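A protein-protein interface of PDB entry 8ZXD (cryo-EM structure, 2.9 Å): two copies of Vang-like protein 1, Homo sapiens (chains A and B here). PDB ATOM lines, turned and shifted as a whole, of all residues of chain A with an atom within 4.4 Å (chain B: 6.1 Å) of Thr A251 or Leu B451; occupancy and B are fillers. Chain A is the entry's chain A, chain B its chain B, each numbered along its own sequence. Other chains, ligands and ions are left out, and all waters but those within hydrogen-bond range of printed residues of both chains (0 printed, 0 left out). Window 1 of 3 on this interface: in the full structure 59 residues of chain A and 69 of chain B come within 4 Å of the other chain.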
ATOM      1  N   PHE A 250     -15.481  16.699 -25.563  1.00  0.00           N
ATOM      2  CA  PHE A 250     -16.570  15.738 -25.491  1.00  0.00           C
ATOM      3  C   PHE A 250     -17.916  16.444 -25.381  1.00  0.00           C
ATOM      4  O   PHE A 250     -18.005  17.622 -25.024  1.00  0.00           O
ATOM      5  CB  PHE A 250     -16.385  14.791 -24.300  1.00  0.00           C
ATOM      6  CG  PHE A 250     -15.043  14.117 -24.262  1.00  0.00           C
ATOM      7  CD1 PHE A 250     -14.778  13.028 -25.075  1.00  0.00           C
ATOM      8  CD2 PHE A 250     -14.049  14.571 -23.414  1.00  0.00           C
ATOM      9  CE1 PHE A 250     -13.545  12.405 -25.043  1.00  0.00           C
ATOM     10  CE2 PHE A 250     -12.813  13.953 -23.377  1.00  0.00           C
ATOM     11  CZ  PHE A 250     -12.561  12.868 -24.193  1.00  0.00           C
ATOM     12  N   THR A 251     -18.971  15.695 -25.696  1.00  0.00           N
ATOM     13  CA  THR A 251     -20.344  16.171 -25.604  1.00  0.00           C
ATOM     14  C   THR A 251     -21.105  15.304 -24.610  1.00  0.00           C
ATOM     15  O   THR A 251     -21.054  14.071 -24.687  1.00  0.00           O
ATOM     16  CB  THR A 251     -21.035  16.141 -26.970  1.00  0.00           C
ATOM     17  OG1 THR A 251     -20.262  16.892 -27.915  1.00  0.00           O
ATOM     18  CG2 THR A 251     -22.430  16.743 -26.876  1.00  0.00           C
ATOM     19  N   LEU A 252     -21.807  15.948 -23.683  1.00  0.00           N
ATOM     20  CA  LEU A 252     -22.572  15.264 -22.648  1.00  0.00           C
ATOM     21  C   LEU A 252     -24.056  15.515 -22.877  1.00  0.00           C
ATOM     22  O   LEU A 252     -24.493  16.670 -22.954  1.00  0.00           O
ATOM     23  CB  LEU A 252     -22.155  15.738 -21.256  1.00  0.00           C
ATOM     24  CG  LEU A 252     -21.086  14.912 -20.534  1.00  0.00           C
ATOM     25  CD1 LEU A 252     -19.756  14.977 -21.269  1.00  0.00           C
ATOM     26  CD2 LEU A 252     -20.930  15.380 -19.096  1.00  0.00           C
ATOM     27  N   GLN A 253     -24.826  14.436 -22.982  1.00  0.00           N
ATOM     28  CA  GLN A 253     -26.274  14.500 -23.121  1.00  0.00           C
ATOM     29  C   GLN A 253     -26.904  14.044 -21.814  1.00  0.00           C
ATOM     30  O   GLN A 253     -26.676  12.912 -21.375  1.00  0.00           O
ATOM     31  CB  GLN A 253     -26.754  13.630 -24.284  1.00  0.00           C
ATOM     32  CG  GLN A 253     -28.241  13.312 -24.247  1.00  0.00           C
ATOM     33  CD  GLN A 253     -28.625  12.215 -25.221  1.00  0.00           C
ATOM     34  OE1 GLN A 253     -27.781  11.686 -25.943  1.00  0.00           O
ATOM     35  NE2 GLN A 253     -29.907  11.868 -25.244  1.00  0.00           N
ATOM     36  N   PHE A 264     -28.098  19.190 -23.865  1.00  0.00           N
ATOM     37  CA  PHE A 264     -26.787  18.890 -24.422  1.00  0.00           C
ATOM     38  C   PHE A 264     -25.789  19.950 -23.981  1.00  0.00           C
ATOM     39  O   PHE A 264     -26.096  21.145 -23.988  1.00  0.00           O
ATOM     40  CB  PHE A 264     -26.833  18.822 -25.952  1.00  0.00           C
ATOM     41  CG  PHE A 264     -27.143  17.455 -26.490  1.00  0.00           C
ATOM     42  CD1 PHE A 264     -28.409  16.912 -26.349  1.00  0.00           C
ATOM     43  CD2 PHE A 264     -26.169  16.713 -27.135  1.00  0.00           C
ATOM     44  CE1 PHE A 264     -28.698  15.655 -26.842  1.00  0.00           C
ATOM     45  CE2 PHE A 264     -26.451  15.454 -27.631  1.00  0.00           C
ATOM     46  CZ  PHE A 264     -27.718  14.924 -27.484  1.00  0.00           C
ATOM     47  N   TYR A 265     -24.593  19.504 -23.599  1.00  0.00           N
ATOM     48  CA  TYR A 265     -23.526  20.402 -23.185  1.00  0.00           C
ATOM     49  C   TYR A 265     -22.217  19.930 -23.799  1.00  0.00           C
ATOM     50  O   TYR A 265     -22.074  18.769 -24.187  1.00  0.00           O
ATOM     51  CB  TYR A 265     -23.401  20.470 -21.656  1.00  0.00           C
ATOM     52  CG  TYR A 265     -24.713  20.705 -20.941  1.00  0.00           C
ATOM     53  CD1 TYR A 265     -25.326  21.950 -20.965  1.00  0.00           C
ATOM     54  CD2 TYR A 265     -25.336  19.679 -20.242  1.00  0.00           C
ATOM     55  CE1 TYR A 265     -26.526  22.167 -20.313  1.00  0.00           C
ATOM     56  CE2 TYR A 265     -26.536  19.888 -19.586  1.00  0.00           C
ATOM     57  CZ  TYR A 265     -27.125  21.133 -19.625  1.00  0.00           C
ATOM     58  OH  TYR A 265     -28.319  21.345 -18.975  1.00  0.00           O
ATOM     59  N   ASN A 493     -24.894  10.688 -20.947  1.00  0.00           N
ATOM     60  CA  ASN A 493     -24.166   9.961 -21.975  1.00  0.00           C
ATOM     61  C   ASN A 493     -23.030  10.836 -22.485  1.00  0.00           C
ATOM     62  O   ASN A 493     -23.226  12.026 -22.750  1.00  0.00           O
ATOM     63  CB  ASN A 493     -25.088   9.591 -23.142  1.00  0.00           C
ATOM     64  CG  ASN A 493     -26.127   8.554 -22.765  1.00  0.00           C
ATOM     65  OD1 ASN A 493     -25.835   7.592 -22.061  1.00  0.00           O
ATOM     66  ND2 ASN A 493     -27.353   8.749 -23.238  1.00  0.00           N
ATOM     67  N   VAL A 494     -21.845  10.248 -22.625  1.00  0.00           N
ATOM     68  CA  VAL A 494     -20.656  10.962 -23.075  1.00  0.00           C
ATOM     69  C   VAL A 494     -20.294  10.474 -24.471  1.00  0.00           C
ATOM     70  O   VAL A 494     -20.188   9.265 -24.705  1.00  0.00           O
ATOM     71  CB  VAL A 494     -19.480  10.769 -22.102  1.00  0.00           C
ATOM     72  CG1 VAL A 494     -18.308  11.648 -22.508  1.00  0.00           C
ATOM     73  CG2 VAL A 494     -19.919  11.080 -20.680  1.00  0.00           C
ATOM     74  N   LYS A 495     -20.104  11.416 -25.395  1.00  0.00           N
ATOM     75  CA  LYS A 495     -19.746  11.102 -26.769  1.00  0.00           C
ATOM     76  C   LYS A 495     -18.558  11.954 -27.194  1.00  0.00           C
ATOM     77  O   LYS A 495     -18.317  13.038 -26.657  1.00  0.00           O
ATOM     78  CB  LYS A 495     -20.923  11.330 -27.730  1.00  0.00           C
ATOM     79  CG  LYS A 495     -22.186  10.566 -27.365  1.00  0.00           C
ATOM     80  CD  LYS A 495     -23.342  10.944 -28.276  1.00  0.00           C
ATOM     81  CE  LYS A 495     -24.635  10.278 -27.835  1.00  0.00           C
ATOM     82  NZ  LYS A 495     -24.531   8.793 -27.859  1.00  0.00           N
ATOM     83  N   ILE A 497     -16.560  14.107 -30.101  1.00  0.00           N
ATOM     84  CA  ILE A 497     -16.845  14.915 -31.293  1.00  0.00           C
ATOM     85  C   ILE A 497     -16.184  14.268 -32.505  1.00  0.00           C
ATOM     86  O   ILE A 497     -14.981  13.950 -32.456  1.00  0.00           O
ATOM     87  CB  ILE A 497     -16.354  16.349 -31.094  1.00  0.00           C
ATOM     88  CG1 ILE A 497     -17.317  17.118 -30.185  1.00  0.00           C
ATOM     89  CG2 ILE A 497     -16.201  17.058 -32.432  1.00  0.00           C
ATOM     90  CD1 ILE A 497     -17.009  18.595 -30.073  1.00  0.00           C
ATOM     91  N   TYR B 284     -23.936  20.185 -34.588  1.00  0.00           N
ATOM     92  CA  TYR B 284     -24.372  18.845 -34.207  1.00  0.00           C
ATOM     93  C   TYR B 284     -25.211  18.871 -32.934  1.00  0.00           C
ATOM     94  O   TYR B 284     -26.226  18.171 -32.838  1.00  0.00           O
ATOM     95  CB  TYR B 284     -23.161  17.929 -34.032  1.00  0.00           C
ATOM     96  CG  TYR B 284     -22.380  17.697 -35.306  1.00  0.00           C
ATOM     97  CD1 TYR B 284     -23.026  17.358 -36.488  1.00  0.00           C
ATOM     98  CD2 TYR B 284     -20.996  17.815 -35.328  1.00  0.00           C
ATOM     99  CE1 TYR B 284     -22.318  17.144 -37.655  1.00  0.00           C
ATOM    100  CE2 TYR B 284     -20.279  17.603 -36.490  1.00  0.00           C
ATOM    101  CZ  TYR B 284     -20.945  17.267 -37.650  1.00  0.00           C
ATOM    102  OH  TYR B 284     -20.234  17.055 -38.809  1.00  0.00           O
ATOM    103  N   LYS B 285     -24.805  19.667 -31.947  1.00  0.00           N
ATOM    104  CA  LYS B 285     -25.488  19.700 -30.662  1.00  0.00           C
ATOM    105  C   LYS B 285     -26.556  20.783 -30.567  1.00  0.00           C
ATOM    106  O   LYS B 285     -27.267  20.837 -29.557  1.00  0.00           O
ATOM    107  CB  LYS B 285     -24.473  19.893 -29.530  1.00  0.00           C
ATOM    108  CG  LYS B 285     -23.639  21.158 -29.652  1.00  0.00           C
ATOM    109  CD  LYS B 285     -22.558  21.210 -28.584  1.00  0.00           C
ATOM    110  CE  LYS B 285     -23.085  21.813 -27.293  1.00  0.00           C
ATOM    111  NZ  LYS B 285     -23.645  23.177 -27.505  1.00  0.00           N
ATOM    112  N   PRO B 449     -31.194  16.787 -31.923  1.00  0.00           N
ATOM    113  CA  PRO B 449     -29.813  16.991 -32.370  1.00  0.00           C
ATOM    114  C   PRO B 449     -29.308  15.831 -33.215  1.00  0.00           C
ATOM    115  O   PRO B 449     -29.821  14.710 -33.166  1.00  0.00           O
ATOM    116  CB  PRO B 449     -29.028  17.104 -31.060  1.00  0.00           C
ATOM    117  CG  PRO B 449     -29.857  16.366 -30.065  1.00  0.00           C
ATOM    118  CD  PRO B 449     -31.284  16.597 -30.465  1.00  0.00           C
ATOM    119  N   THR B 450     -28.277  16.129 -34.008  1.00  0.00           N
ATOM    120  CA  THR B 450     -27.674  15.121 -34.874  1.00  0.00           C
ATOM    121  C   THR B 450     -27.007  14.007 -34.075  1.00  0.00           C
ATOM    122  O   THR B 450     -27.064  12.840 -34.478  1.00  0.00           O
ATOM    123  CB  THR B 450     -26.656  15.780 -35.808  1.00  0.00           C
ATOM    124  OG1 THR B 450     -27.261  16.900 -36.466  1.00  0.00           O
ATOM    125  CG2 THR B 450     -26.159  14.789 -36.850  1.00  0.00           C
ATOM    126  N   LEU B 451     -26.380  14.343 -32.945  1.00  0.00           N
ATOM    127  CA  LEU B 451     -25.612  13.360 -32.188  1.00  0.00           C
ATOM    128  C   LEU B 451     -26.484  12.272 -31.573  1.00  0.00           C
ATOM    129  O   LEU B 451     -25.951  11.245 -31.138  1.00  0.00           O
ATOM    130  CB  LEU B 451     -24.806  14.059 -31.092  1.00  0.00           C
ATOM    131  CG  LEU B 451     -23.649  14.937 -31.571  1.00  0.00           C
ATOM    132  CD1 LEU B 451     -23.014  15.677 -30.405  1.00  0.00           C
ATOM    133  CD2 LEU B 451     -22.612  14.104 -32.310  1.00  0.00           C
ATOM    134  N   GLN B 452     -27.803  12.471 -31.520  1.00  0.00           N
ATOM    135  CA  GLN B 452     -28.681  11.461 -30.938  1.00  0.00           C
ATOM    136  C   GLN B 452     -28.683  10.177 -31.761  1.00  0.00           C
ATOM    137  O   GLN B 452     -28.708   9.075 -31.201  1.00  0.00           O
ATOM    138  CB  GLN B 452     -30.100  12.014 -30.804  1.00  0.00           C
ATOM    139  CG  GLN B 452     -30.373  12.709 -29.481  1.00  0.00           C
ATOM    140  CD  GLN B 452     -31.779  13.268 -29.396  1.00  0.00           C
ATOM    141  OE1 GLN B 452     -32.566  13.144 -30.333  1.00  0.00           O
ATOM    142  NE2 GLN B 452     -32.102  13.888 -28.266  1.00  0.00           N
ATOM    143  N   TYR B 453     -28.655  10.297 -33.086  1.00  0.00           N
ATOM    144  CA  TYR B 453     -28.756   9.140 -33.965  1.00  0.00           C
ATOM    145  C   TYR B 453     -27.398   8.444 -34.074  1.00  0.00           C
ATOM    146  O   TYR B 453     -26.445   8.763 -33.358  1.00  0.00           O
ATOM    147  CB  TYR B 453     -29.297   9.562 -35.328  1.00  0.00           C
ATOM    148  CG  TYR B 453     -30.580  10.359 -35.250  1.00  0.00           C
ATOM    149  CD1 TYR B 453     -31.785   9.741 -34.942  1.00  0.00           C
ATOM    150  CD2 TYR B 453     -30.586  11.728 -35.479  1.00  0.00           C
ATOM    151  CE1 TYR B 453     -32.960  10.464 -34.868  1.00  0.00           C
ATOM    152  CE2 TYR B 453     -31.755  12.459 -35.407  1.00  0.00           C
ATOM    153  CZ  TYR B 453     -32.940  11.823 -35.101  1.00  0.00           C
ATOM    154  OH  TYR B 453     -34.107  12.546 -35.028  1.00  0.00           O
ATOM    155  N   ASP B 454     -27.302   7.476 -34.983  1.00  0.00           N
ATOM    156  CA  ASP B 454     -26.092   6.682 -35.127  1.00  0.00           C
ATOM    157  C   ASP B 454     -24.986   7.496 -35.798  1.00  0.00           C
ATOM    158  O   ASP B 454     -25.211   8.576 -36.354  1.00  0.00           O
ATOM    159  CB  ASP B 454     -26.379   5.411 -35.927  1.00  0.00           C
ATOM    160  CG  ASP B 454     -27.164   5.684 -37.195  1.00  0.00           C
ATOM    161  OD1 ASP B 454     -27.614   6.833 -37.381  1.00  0.00           O
ATOM    162  OD2 ASP B 454     -27.332   4.748 -38.004  1.00  0.00           O
ATOM    163  N   TRP B 458     -24.445  11.120 -39.711  1.00  0.00           N
ATOM    164  CA  TRP B 458     -23.756  12.371 -39.989  1.00  0.00           C
ATOM    165  C   TRP B 458     -22.432  12.114 -40.698  1.00  0.00           C
ATOM    166  O   TRP B 458     -21.776  11.092 -40.482  1.00  0.00           O
ATOM    167  CB  TRP B 458     -23.516  13.165 -38.702  1.00  0.00           C
ATOM    168  CG  TRP B 458     -22.656  12.471 -37.684  1.00  0.00           C
ATOM    169  CD1 TRP B 458     -21.303  12.297 -37.731  1.00  0.00           C
ATOM    170  CD2 TRP B 458     -23.093  11.872 -36.456  1.00  0.00           C
ATOM    171  NE1 TRP B 458     -20.873  11.620 -36.617  1.00  0.00           N
ATOM    172  CE2 TRP B 458     -21.951  11.349 -35.817  1.00  0.00           C
ATOM    173  CE3 TRP B 458     -24.338  11.725 -35.839  1.00  0.00           C
ATOM    174  CZ2 TRP B 458     -22.017  10.692 -34.591  1.00  0.00           C
ATOM    175  CZ3 TRP B 458     -24.401  11.070 -34.621  1.00  0.00           C
ATOM    176  CH2 TRP B 458     -23.249  10.561 -34.011  1.00  0.00           C
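Thr A251 touches Leu B451 (CG2 to CD1, 3.7 Å).
Phe A264 touches Pro B449.
Phe A264 touches Gln B452.
Leu B451 touches Lys A495 (O to CE, 3.7 Å).
Hydrophobic or aromatic side chains of chain A that line the printed part of chain B: Phe A264.
Printed residues of chain B that touch a printed residue of chain A: Pro B449, Leu B451 and Gln B452.
Among the printed residues, 4 pairs touch across the chains.
Thr A251 touches just one residue of chain B: Leu B451 (3.7 Å).
Leu A252 touches none of the printed residues of chain B.
Of the printed residues of chain B, Phe A264 touches Pro B449 (3.5 Å) and Gln B452 (3.99 Å).
Of the printed residues of chain B, Lys A495 touches Leu B451.
Leu B451 touches two residues of chain A.
The nearest residue of chain B that does not touch Thr A251 is Lys B285 (4.6 Å).
The nearest residue of chain A that does not touch Leu B451 is Phe A264 (4.1 Å).
The nearest printed residue of chain B that does not touch Phe A264 is Leu B451 (4.1 Å).
The backbone NH (N) of Thr A251 sits at hydrogen-bond distance from the backbone carbonyl oxygen (O) of Lys A495.
No position is printed for both chains.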
